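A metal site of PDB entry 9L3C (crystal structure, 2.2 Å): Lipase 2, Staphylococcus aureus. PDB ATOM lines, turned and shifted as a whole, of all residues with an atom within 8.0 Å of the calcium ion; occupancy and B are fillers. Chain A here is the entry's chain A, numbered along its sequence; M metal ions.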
ATOM      1  N   LYS A  51       6.239  26.573  -1.912  1.00  0.00           N
ATOM      2  CA  LYS A  51       6.007  25.412  -2.753  1.00  0.00           C
ATOM      3  C   LYS A  51       5.482  24.242  -1.935  1.00  0.00           C
ATOM      4  O   LYS A  51       4.567  23.581  -2.369  1.00  0.00           O
ATOM      5  CB  LYS A  51       7.278  25.091  -3.533  1.00  0.00           C
ATOM      6  CG  LYS A  51       7.655  26.137  -4.561  1.00  0.00           C
ATOM      7  CD  LYS A  51       8.748  25.726  -5.493  1.00  0.00           C
ATOM      8  CE  LYS A  51       9.150  26.869  -6.390  1.00  0.00           C
ATOM      9  NZ  LYS A  51      10.062  26.382  -7.441  1.00  0.00           N
ATOM     10  N   SER A 283      22.824  21.555 -11.424  1.00  0.00           N
ATOM     11  CA  SER A 283      22.153  22.651 -12.098  1.00  0.00           C
ATOM     12  C   SER A 283      23.168  23.411 -12.950  1.00  0.00           C
ATOM     13  O   SER A 283      23.006  24.608 -13.194  1.00  0.00           O
ATOM     14  CB  SER A 283      21.500  23.542 -11.055  1.00  0.00           C
ATOM     15  OG  SER A 283      20.829  24.624 -11.660  1.00  0.00           O
ATOM     16  N   ASP A 295      22.772  26.488 -15.199  1.00  0.00           N
ATOM     17  CA  ASP A 295      21.588  26.378 -16.018  1.00  0.00           C
ATOM     18  C   ASP A 295      20.741  27.630 -15.826  1.00  0.00           C
ATOM     19  O   ASP A 295      20.678  28.169 -14.723  1.00  0.00           O
ATOM     20  CB  ASP A 295      20.761  25.163 -15.608  1.00  0.00           C
ATOM     21  CG  ASP A 295      21.390  23.808 -15.948  1.00  0.00           C
ATOM     22  OD1 ASP A 295      22.446  23.795 -16.637  1.00  0.00           O
ATOM     23  OD2 ASP A 295      20.821  22.779 -15.510  1.00  0.00           O
ATOM     24  N   LEU A 296      20.096  28.094 -16.906  1.00  0.00           N
ATOM     25  CA  LEU A 296      18.917  28.931 -16.732  1.00  0.00           C
ATOM     26  C   LEU A 296      18.013  28.212 -15.738  1.00  0.00           C
ATOM     27  O   LEU A 296      17.757  27.008 -15.879  1.00  0.00           O
ATOM     28  CB  LEU A 296      18.204  29.159 -18.069  1.00  0.00           C
ATOM     29  CG  LEU A 296      18.395  30.524 -18.733  1.00  0.00           C
ATOM     30  CD1 LEU A 296      17.954  31.686 -17.820  1.00  0.00           C
ATOM     31  CD2 LEU A 296      19.849  30.695 -19.214  1.00  0.00           C
ATOM     32  N   GLY A 297      17.586  28.917 -14.698  1.00  0.00           N
ATOM     33  CA  GLY A 297      16.789  28.267 -13.671  1.00  0.00           C
ATOM     34  C   GLY A 297      17.571  28.022 -12.381  1.00  0.00           C
ATOM     35  O   GLY A 297      16.976  27.722 -11.342  1.00  0.00           O
ATOM     36  N   THR A 298      18.905  28.135 -12.449  1.00  0.00           N
ATOM     37  CA  THR A 298      19.705  28.254 -11.236  1.00  0.00           C
ATOM     38  C   THR A 298      19.321  29.561 -10.561  1.00  0.00           C
ATOM     39  O   THR A 298      19.466  30.608 -11.173  1.00  0.00           O
ATOM     40  CB  THR A 298      21.211  28.272 -11.545  1.00  0.00           C
ATOM     41  OG1 THR A 298      21.560  27.128 -12.323  1.00  0.00           O
ATOM     42  CG2 THR A 298      22.049  28.270 -10.297  1.00  0.00           C
ATOM     43  N   PHE A 299      18.819  29.514  -9.333  1.00  0.00           N
ATOM     44  CA  PHE A 299      18.498  30.713  -8.583  1.00  0.00           C
ATOM     45  C   PHE A 299      19.631  31.737  -8.735  1.00  0.00           C
ATOM     46  O   PHE A 299      20.786  31.408  -8.474  1.00  0.00           O
ATOM     47  CB  PHE A 299      18.234  30.326  -7.127  1.00  0.00           C
ATOM     48  CG  PHE A 299      17.657  31.455  -6.314  1.00  0.00           C
ATOM     49  CD1 PHE A 299      16.425  31.971  -6.668  1.00  0.00           C
ATOM     50  CD2 PHE A 299      18.350  32.010  -5.259  1.00  0.00           C
ATOM     51  CE1 PHE A 299      15.892  33.021  -5.954  1.00  0.00           C
ATOM     52  CE2 PHE A 299      17.804  33.058  -4.551  1.00  0.00           C
ATOM     53  CZ  PHE A 299      16.592  33.579  -4.913  1.00  0.00           C
ATOM     54  N   PHE A 300      19.274  32.959  -9.143  1.00  0.00           N
ATOM     55  CA  PHE A 300      20.220  33.921  -9.714  1.00  0.00           C
ATOM     56  C   PHE A 300      21.300  34.303  -8.709  1.00  0.00           C
ATOM     57  O   PHE A 300      22.417  34.643  -9.095  1.00  0.00           O
ATOM     58  CB  PHE A 300      19.527  35.187 -10.208  1.00  0.00           C
ATOM     59  CG  PHE A 300      18.839  35.999  -9.133  1.00  0.00           C
ATOM     60  CD1 PHE A 300      17.620  35.595  -8.608  1.00  0.00           C
ATOM     61  CD2 PHE A 300      19.427  37.149  -8.634  1.00  0.00           C
ATOM     62  CE1 PHE A 300      17.002  36.320  -7.600  1.00  0.00           C
ATOM     63  CE2 PHE A 300      18.810  37.874  -7.627  1.00  0.00           C
ATOM     64  CZ  PHE A 300      17.594  37.460  -7.121  1.00  0.00           C
ATOM     65  N   MET A 302      23.087  32.521  -7.040  1.00  0.00           N
ATOM     66  CA  MET A 302      24.218  31.593  -7.106  1.00  0.00           C
ATOM     67  C   MET A 302      24.908  31.649  -8.460  1.00  0.00           C
ATOM     68  O   MET A 302      25.752  30.810  -8.769  1.00  0.00           O
ATOM     69  CB  MET A 302      23.704  30.178  -6.841  1.00  0.00           C
ATOM     70  CG  MET A 302      23.259  30.021  -5.436  1.00  0.00           C
ATOM     71  SD  MET A 302      22.666  28.367  -5.101  1.00  0.00           S
ATOM     72  CE  MET A 302      21.281  28.207  -6.227  1.00  0.00           C
ATOM     73  N   ASP A 321      25.495  22.504  -7.946  1.00  0.00           N
ATOM     74  CA  ASP A 321      24.097  22.838  -7.770  1.00  0.00           C
ATOM     75  C   ASP A 321      23.907  24.343  -7.620  1.00  0.00           C
ATOM     76  O   ASP A 321      22.861  24.773  -7.165  1.00  0.00           O
ATOM     77  CB  ASP A 321      23.476  22.144  -6.552  1.00  0.00           C
ATOM     78  CG  ASP A 321      23.958  22.660  -5.210  1.00  0.00           C
ATOM     79  OD1 ASP A 321      24.812  23.571  -5.195  1.00  0.00           O
ATOM     80  OD2 ASP A 321      23.515  22.103  -4.178  1.00  0.00           O
ATOM     81  N   GLY A 360      18.708  19.062 -12.611  1.00  0.00           N
ATOM     82  CA  GLY A 360      18.032  20.342 -12.688  1.00  0.00           C
ATOM     83  C   GLY A 360      17.674  20.942 -11.328  1.00  0.00           C
ATOM     84  O   GLY A 360      17.121  22.035 -11.276  1.00  0.00           O
ATOM     85  N   TRP A 361      17.950  20.248 -10.221  1.00  0.00           N
ATOM     86  CA  TRP A 361      17.721  20.850  -8.920  1.00  0.00           C
ATOM     87  C   TRP A 361      18.946  21.640  -8.490  1.00  0.00           C
ATOM     88  O   TRP A 361      20.031  21.074  -8.435  1.00  0.00           O
ATOM     89  CB  TRP A 361      17.422  19.812  -7.859  1.00  0.00           C
ATOM     90  CG  TRP A 361      16.107  19.121  -8.007  1.00  0.00           C
ATOM     91  CD1 TRP A 361      15.561  18.607  -9.139  1.00  0.00           C
ATOM     92  CD2 TRP A 361      15.225  18.787  -6.920  1.00  0.00           C
ATOM     93  NE1 TRP A 361      14.371  18.003  -8.821  1.00  0.00           N
ATOM     94  CE2 TRP A 361      14.150  18.085  -7.481  1.00  0.00           C
ATOM     95  CE3 TRP A 361      15.244  19.017  -5.536  1.00  0.00           C
ATOM     96  CZ2 TRP A 361      13.093  17.603  -6.700  1.00  0.00           C
ATOM     97  CZ3 TRP A 361      14.203  18.544  -4.772  1.00  0.00           C
ATOM     98  CH2 TRP A 361      13.143  17.851  -5.350  1.00  0.00           C
ATOM     99  N   ASP A 362      18.772  22.921  -8.180  1.00  0.00           N
ATOM    100  CA  ASP A 362      19.874  23.695  -7.650  1.00  0.00           C
ATOM    101  C   ASP A 362      19.806  23.628  -6.132  1.00  0.00           C
ATOM    102  O   ASP A 362      18.880  23.030  -5.565  1.00  0.00           O
ATOM    103  CB  ASP A 362      19.887  25.134  -8.192  1.00  0.00           C
ATOM    104  CG  ASP A 362      18.700  26.005  -7.786  1.00  0.00           C
ATOM    105  OD1 ASP A 362      18.160  25.821  -6.650  1.00  0.00           O
ATOM    106  OD2 ASP A 362      18.350  26.905  -8.620  1.00  0.00           O
ATOM    107  N   HIS A 363      20.821  24.227  -5.511  1.00  0.00           N
ATOM    108  CA  HIS A 363      21.001  24.221  -4.067  1.00  0.00           C
ATOM    109  C   HIS A 363      19.699  24.551  -3.340  1.00  0.00           C
ATOM    110  O   HIS A 363      19.409  23.911  -2.333  1.00  0.00           O
ATOM    111  CB  HIS A 363      22.067  25.236  -3.665  1.00  0.00           C
ATOM    112  CG  HIS A 363      22.559  25.016  -2.298  1.00  0.00           C
ATOM    113  ND1 HIS A 363      23.334  23.933  -1.963  1.00  0.00           N
ATOM    114  CD2 HIS A 363      22.396  25.715  -1.188  1.00  0.00           C
ATOM    115  CE1 HIS A 363      23.625  23.992  -0.688  1.00  0.00           C
ATOM    116  NE2 HIS A 363      23.056  25.067  -0.189  1.00  0.00           N
ATOM    117  N   VAL A 364      18.951  25.547  -3.830  1.00  0.00           N
ATOM    118  CA  VAL A 364      17.815  26.033  -3.074  1.00  0.00           C
ATOM    119  C   VAL A 364      16.522  25.385  -3.537  1.00  0.00           C
ATOM    120  O   VAL A 364      15.519  25.404  -2.813  1.00  0.00           O
ATOM    121  CB  VAL A 364      17.713  27.576  -3.044  1.00  0.00           C
ATOM    122  CG1 VAL A 364      18.975  28.198  -2.451  1.00  0.00           C
ATOM    123  CG2 VAL A 364      17.408  28.178  -4.412  1.00  0.00           C
ATOM    124  N   ASP A 365      16.516  24.734  -4.715  1.00  0.00           N
ATOM    125  CA  ASP A 365      15.349  23.952  -5.076  1.00  0.00           C
ATOM    126  C   ASP A 365      15.032  22.892  -4.002  1.00  0.00           C
ATOM    127  O   ASP A 365      13.864  22.575  -3.787  1.00  0.00           O
ATOM    128  CB  ASP A 365      15.463  23.390  -6.478  1.00  0.00           C
ATOM    129  CG  ASP A 365      15.513  24.459  -7.559  1.00  0.00           C
ATOM    130  OD1 ASP A 365      14.712  25.418  -7.467  1.00  0.00           O
ATOM    131  OD2 ASP A 365      16.326  24.314  -8.506  1.00  0.00           O
ATOM    132  N   PHE A 366      16.019  22.385  -3.271  1.00  0.00           N
ATOM    133  CA  PHE A 366      15.733  21.387  -2.248  1.00  0.00           C
ATOM    134  C   PHE A 366      14.803  21.925  -1.151  1.00  0.00           C
ATOM    135  O   PHE A 366      14.104  21.142  -0.500  1.00  0.00           O
ATOM    136  CB  PHE A 366      17.025  20.880  -1.614  1.00  0.00           C
ATOM    137  CG  PHE A 366      17.781  19.917  -2.488  1.00  0.00           C
ATOM    138  CD1 PHE A 366      17.418  18.582  -2.519  1.00  0.00           C
ATOM    139  CD2 PHE A 366      18.785  20.370  -3.328  1.00  0.00           C
ATOM    140  CE1 PHE A 366      18.059  17.703  -3.375  1.00  0.00           C
ATOM    141  CE2 PHE A 366      19.421  19.495  -4.192  1.00  0.00           C
ATOM    142  CZ  PHE A 366      19.075  18.162  -4.194  1.00  0.00           C
ATOM    143  N   VAL A 369      12.554  27.524  -2.285  1.00  0.00           N
ATOM    144  CA  VAL A 369      12.491  28.964  -2.151  1.00  0.00           C
ATOM    145  C   VAL A 369      12.820  29.619  -3.495  1.00  0.00           C
ATOM    146  O   VAL A 369      12.844  30.848  -3.582  1.00  0.00           O
ATOM    147  CB  VAL A 369      13.420  29.495  -1.042  1.00  0.00           C
ATOM    148  CG1 VAL A 369      13.107  28.885   0.313  1.00  0.00           C
ATOM    149  CG2 VAL A 369      14.874  29.293  -1.387  1.00  0.00           C
ATOM    150  N   ASP A 370      13.082  28.831  -4.528  1.00  0.00           N
ATOM    151  CA  ASP A 370      13.310  29.426  -5.843  1.00  0.00           C
ATOM    152  C   ASP A 370      11.952  29.704  -6.496  1.00  0.00           C
ATOM    153  O   ASP A 370      11.464  28.894  -7.277  1.00  0.00           O
ATOM    154  CB  ASP A 370      14.238  28.548  -6.687  1.00  0.00           C
ATOM    155  CG  ASP A 370      14.664  29.189  -7.992  1.00  0.00           C
ATOM    156  OD1 ASP A 370      14.084  30.216  -8.353  1.00  0.00           O
ATOM    157  OD2 ASP A 370      15.576  28.651  -8.646  1.00  0.00           O
ATOM    158  N   PHE A 371      11.337  30.841  -6.178  1.00  0.00           N
ATOM    159  CA  PHE A 371      10.016  31.164  -6.718  1.00  0.00           C
ATOM    160  C   PHE A 371      10.125  31.529  -8.196  1.00  0.00           C
ATOM    161  O   PHE A 371       9.118  31.502  -8.891  1.00  0.00           O
ATOM    162  CB  PHE A 371       9.367  32.309  -5.945  1.00  0.00           C
ATOM    163  CG  PHE A 371      10.185  33.570  -5.945  1.00  0.00           C
ATOM    164  CD1 PHE A 371      11.161  33.779  -4.987  1.00  0.00           C
ATOM    165  CD2 PHE A 371      10.057  34.499  -6.977  1.00  0.00           C
ATOM    166  CE1 PHE A 371      11.950  34.908  -5.007  1.00  0.00           C
ATOM    167  CE2 PHE A 371      10.854  35.635  -6.999  1.00  0.00           C
ATOM    168  CZ  PHE A 371      11.807  35.829  -6.023  1.00  0.00           C
ATOM    169  N   LEU A 372      11.348  31.846  -8.665  1.00  0.00           N
ATOM    170  CA  LEU A 372      11.613  32.112 -10.079  1.00  0.00           C
ATOM    171  C   LEU A 372      11.513  30.859 -10.951  1.00  0.00           C
ATOM    172  O   LEU A 372      11.390  31.012 -12.160  1.00  0.00           O
ATOM    173  CB  LEU A 372      13.010  32.737 -10.243  1.00  0.00           C
ATOM    174  CG  LEU A 372      13.176  34.254 -10.078  1.00  0.00           C
ATOM    175  CD1 LEU A 372      11.839  34.938  -9.947  1.00  0.00           C
ATOM    176  CD2 LEU A 372      14.061  34.614  -8.900  1.00  0.00           C
ATOM    177  N   ASP A 373      11.616  29.633 -10.401  1.00  0.00           N
ATOM    178  CA  ASP A 373      11.838  28.431 -11.208  1.00  0.00           C
ATOM    179  C   ASP A 373      10.562  27.576 -11.232  1.00  0.00           C
ATOM    180  O   ASP A 373      10.280  26.845 -10.285  1.00  0.00           O
ATOM    181  CB  ASP A 373      13.040  27.638 -10.682  1.00  0.00           C
ATOM    182  CG  ASP A 373      13.509  26.457 -11.533  1.00  0.00           C
ATOM    183  OD1 ASP A 373      12.793  26.096 -12.509  1.00  0.00           O
ATOM    184  OD2 ASP A 373      14.603  25.904 -11.242  1.00  0.00           O
ATOM    185  N   PHE A 374       9.823  27.663 -12.348  1.00  0.00           N
ATOM    186  CA  PHE A 374       8.493  27.077 -12.476  1.00  0.00           C
ATOM    187  C   PHE A 374       8.597  25.573 -12.799  1.00  0.00           C
ATOM    188  O   PHE A 374       7.660  24.829 -12.553  1.00  0.00           O
ATOM    189  CB  PHE A 374       7.649  27.832 -13.519  1.00  0.00           C
ATOM    190  CG  PHE A 374       7.701  29.351 -13.462  1.00  0.00           C
ATOM    191  CD1 PHE A 374       7.293  30.054 -12.336  1.00  0.00           C
ATOM    192  CD2 PHE A 374       8.093  30.079 -14.584  1.00  0.00           C
ATOM    193  CE1 PHE A 374       7.303  31.456 -12.310  1.00  0.00           C
ATOM    194  CE2 PHE A 374       8.100  31.469 -14.563  1.00  0.00           C
ATOM    195  CZ  PHE A 374       7.717  32.159 -13.419  1.00  0.00           C
ATOM    196  N   LYS A 375       9.743  25.141 -13.349  1.00  0.00           N
ATOM    197  CA  LYS A 375      10.047  23.733 -13.580  1.00  0.00           C
ATOM    198  C   LYS A 375       9.997  22.929 -12.277  1.00  0.00           C
ATOM    199  O   LYS A 375       9.653  21.740 -12.276  1.00  0.00           O
ATOM    200  CB  LYS A 375      11.434  23.559 -14.221  1.00  0.00           C
ATOM    201  CG  LYS A 375      11.605  23.930 -15.693  1.00  0.00           C
ATOM    202  CD  LYS A 375      12.839  23.289 -16.378  1.00  0.00           C
ATOM    203  CE  LYS A 375      14.063  24.183 -16.530  1.00  0.00           C
ATOM    204  NZ  LYS A 375      14.624  24.654 -15.228  1.00  0.00           N
ATOM    205  N   ARG A 376      10.346  23.557 -11.155  1.00  0.00           N
ATOM    206  CA  ARG A 376      10.370  22.848  -9.875  1.00  0.00           C
ATOM    207  C   ARG A 376       9.074  23.115  -9.118  1.00  0.00           C
ATOM    208  O   ARG A 376       8.923  24.167  -8.495  1.00  0.00           O
ATOM    209  CB  ARG A 376      11.571  23.311  -9.050  1.00  0.00           C
ATOM    210  CG  ARG A 376      12.897  23.226  -9.776  1.00  0.00           C
ATOM    211  CD  ARG A 376      13.545  21.870  -9.557  1.00  0.00           C
ATOM    212  NE  ARG A 376      12.825  20.750 -10.142  1.00  0.00           N
ATOM    213  CZ  ARG A 376      12.974  20.324 -11.402  1.00  0.00           C
ATOM    214  NH1 ARG A 376      12.313  19.254 -11.810  1.00  0.00           N
ATOM    215  NH2 ARG A 376      13.772  20.971 -12.233  1.00  0.00           N
HETATM  216 CA    CA M   1      16.201  26.381  -9.582  1.00  0.00          CA
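O of Asp 373 lies within hydrogen-bond range of NZ of Lys 51 (2.9 Å).
The side-chain carboxylate (OD1) of Asp 362 is in hydrogen-bond range of the backbone NH (N) of Val 364 (2.9 Å).
OD2 of Asp 370 lies close to N of Phe 299 (3.4 Å).
The side-chain carboxylate (OD2) of Asp 362 lies close to the backbone NH (N) of Phe 299 (2.7 Å).
OD1 of Asp 370 sits close to N of Leu 372 (3.2 Å).
The side-chain amino group of Lys 51 sits at hydrogen-bond distance from the backbone carbonyl oxygen of Asp 370 (2.9 Å).
The side-chain amino group (NZ) of Lys 375 is in salt-bridge range of the side-chain carboxylate (OD1) of Asp 373 (3.6 Å).
The nearest printed residue that does not touch the calcium ion is Phe 299 (4.1 Å).
The calcium ion is bound by the side-chain carboxylate (OD2) of Asp 365 (2.3 Å), the backbone carbonyl oxygen (O) of Gly 297 (2.3 Å), the side-chain carboxylate (OD2) of Asp 373 (2.4 Å), the side-chain carboxylate (OD2) of Asp 362 (2.4 Å), the side-chain carboxylate (OD2) of Asp 370 (2.5 Å) and the side-chain carboxylate (OD1) of Asp 365 (2.8 Å).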
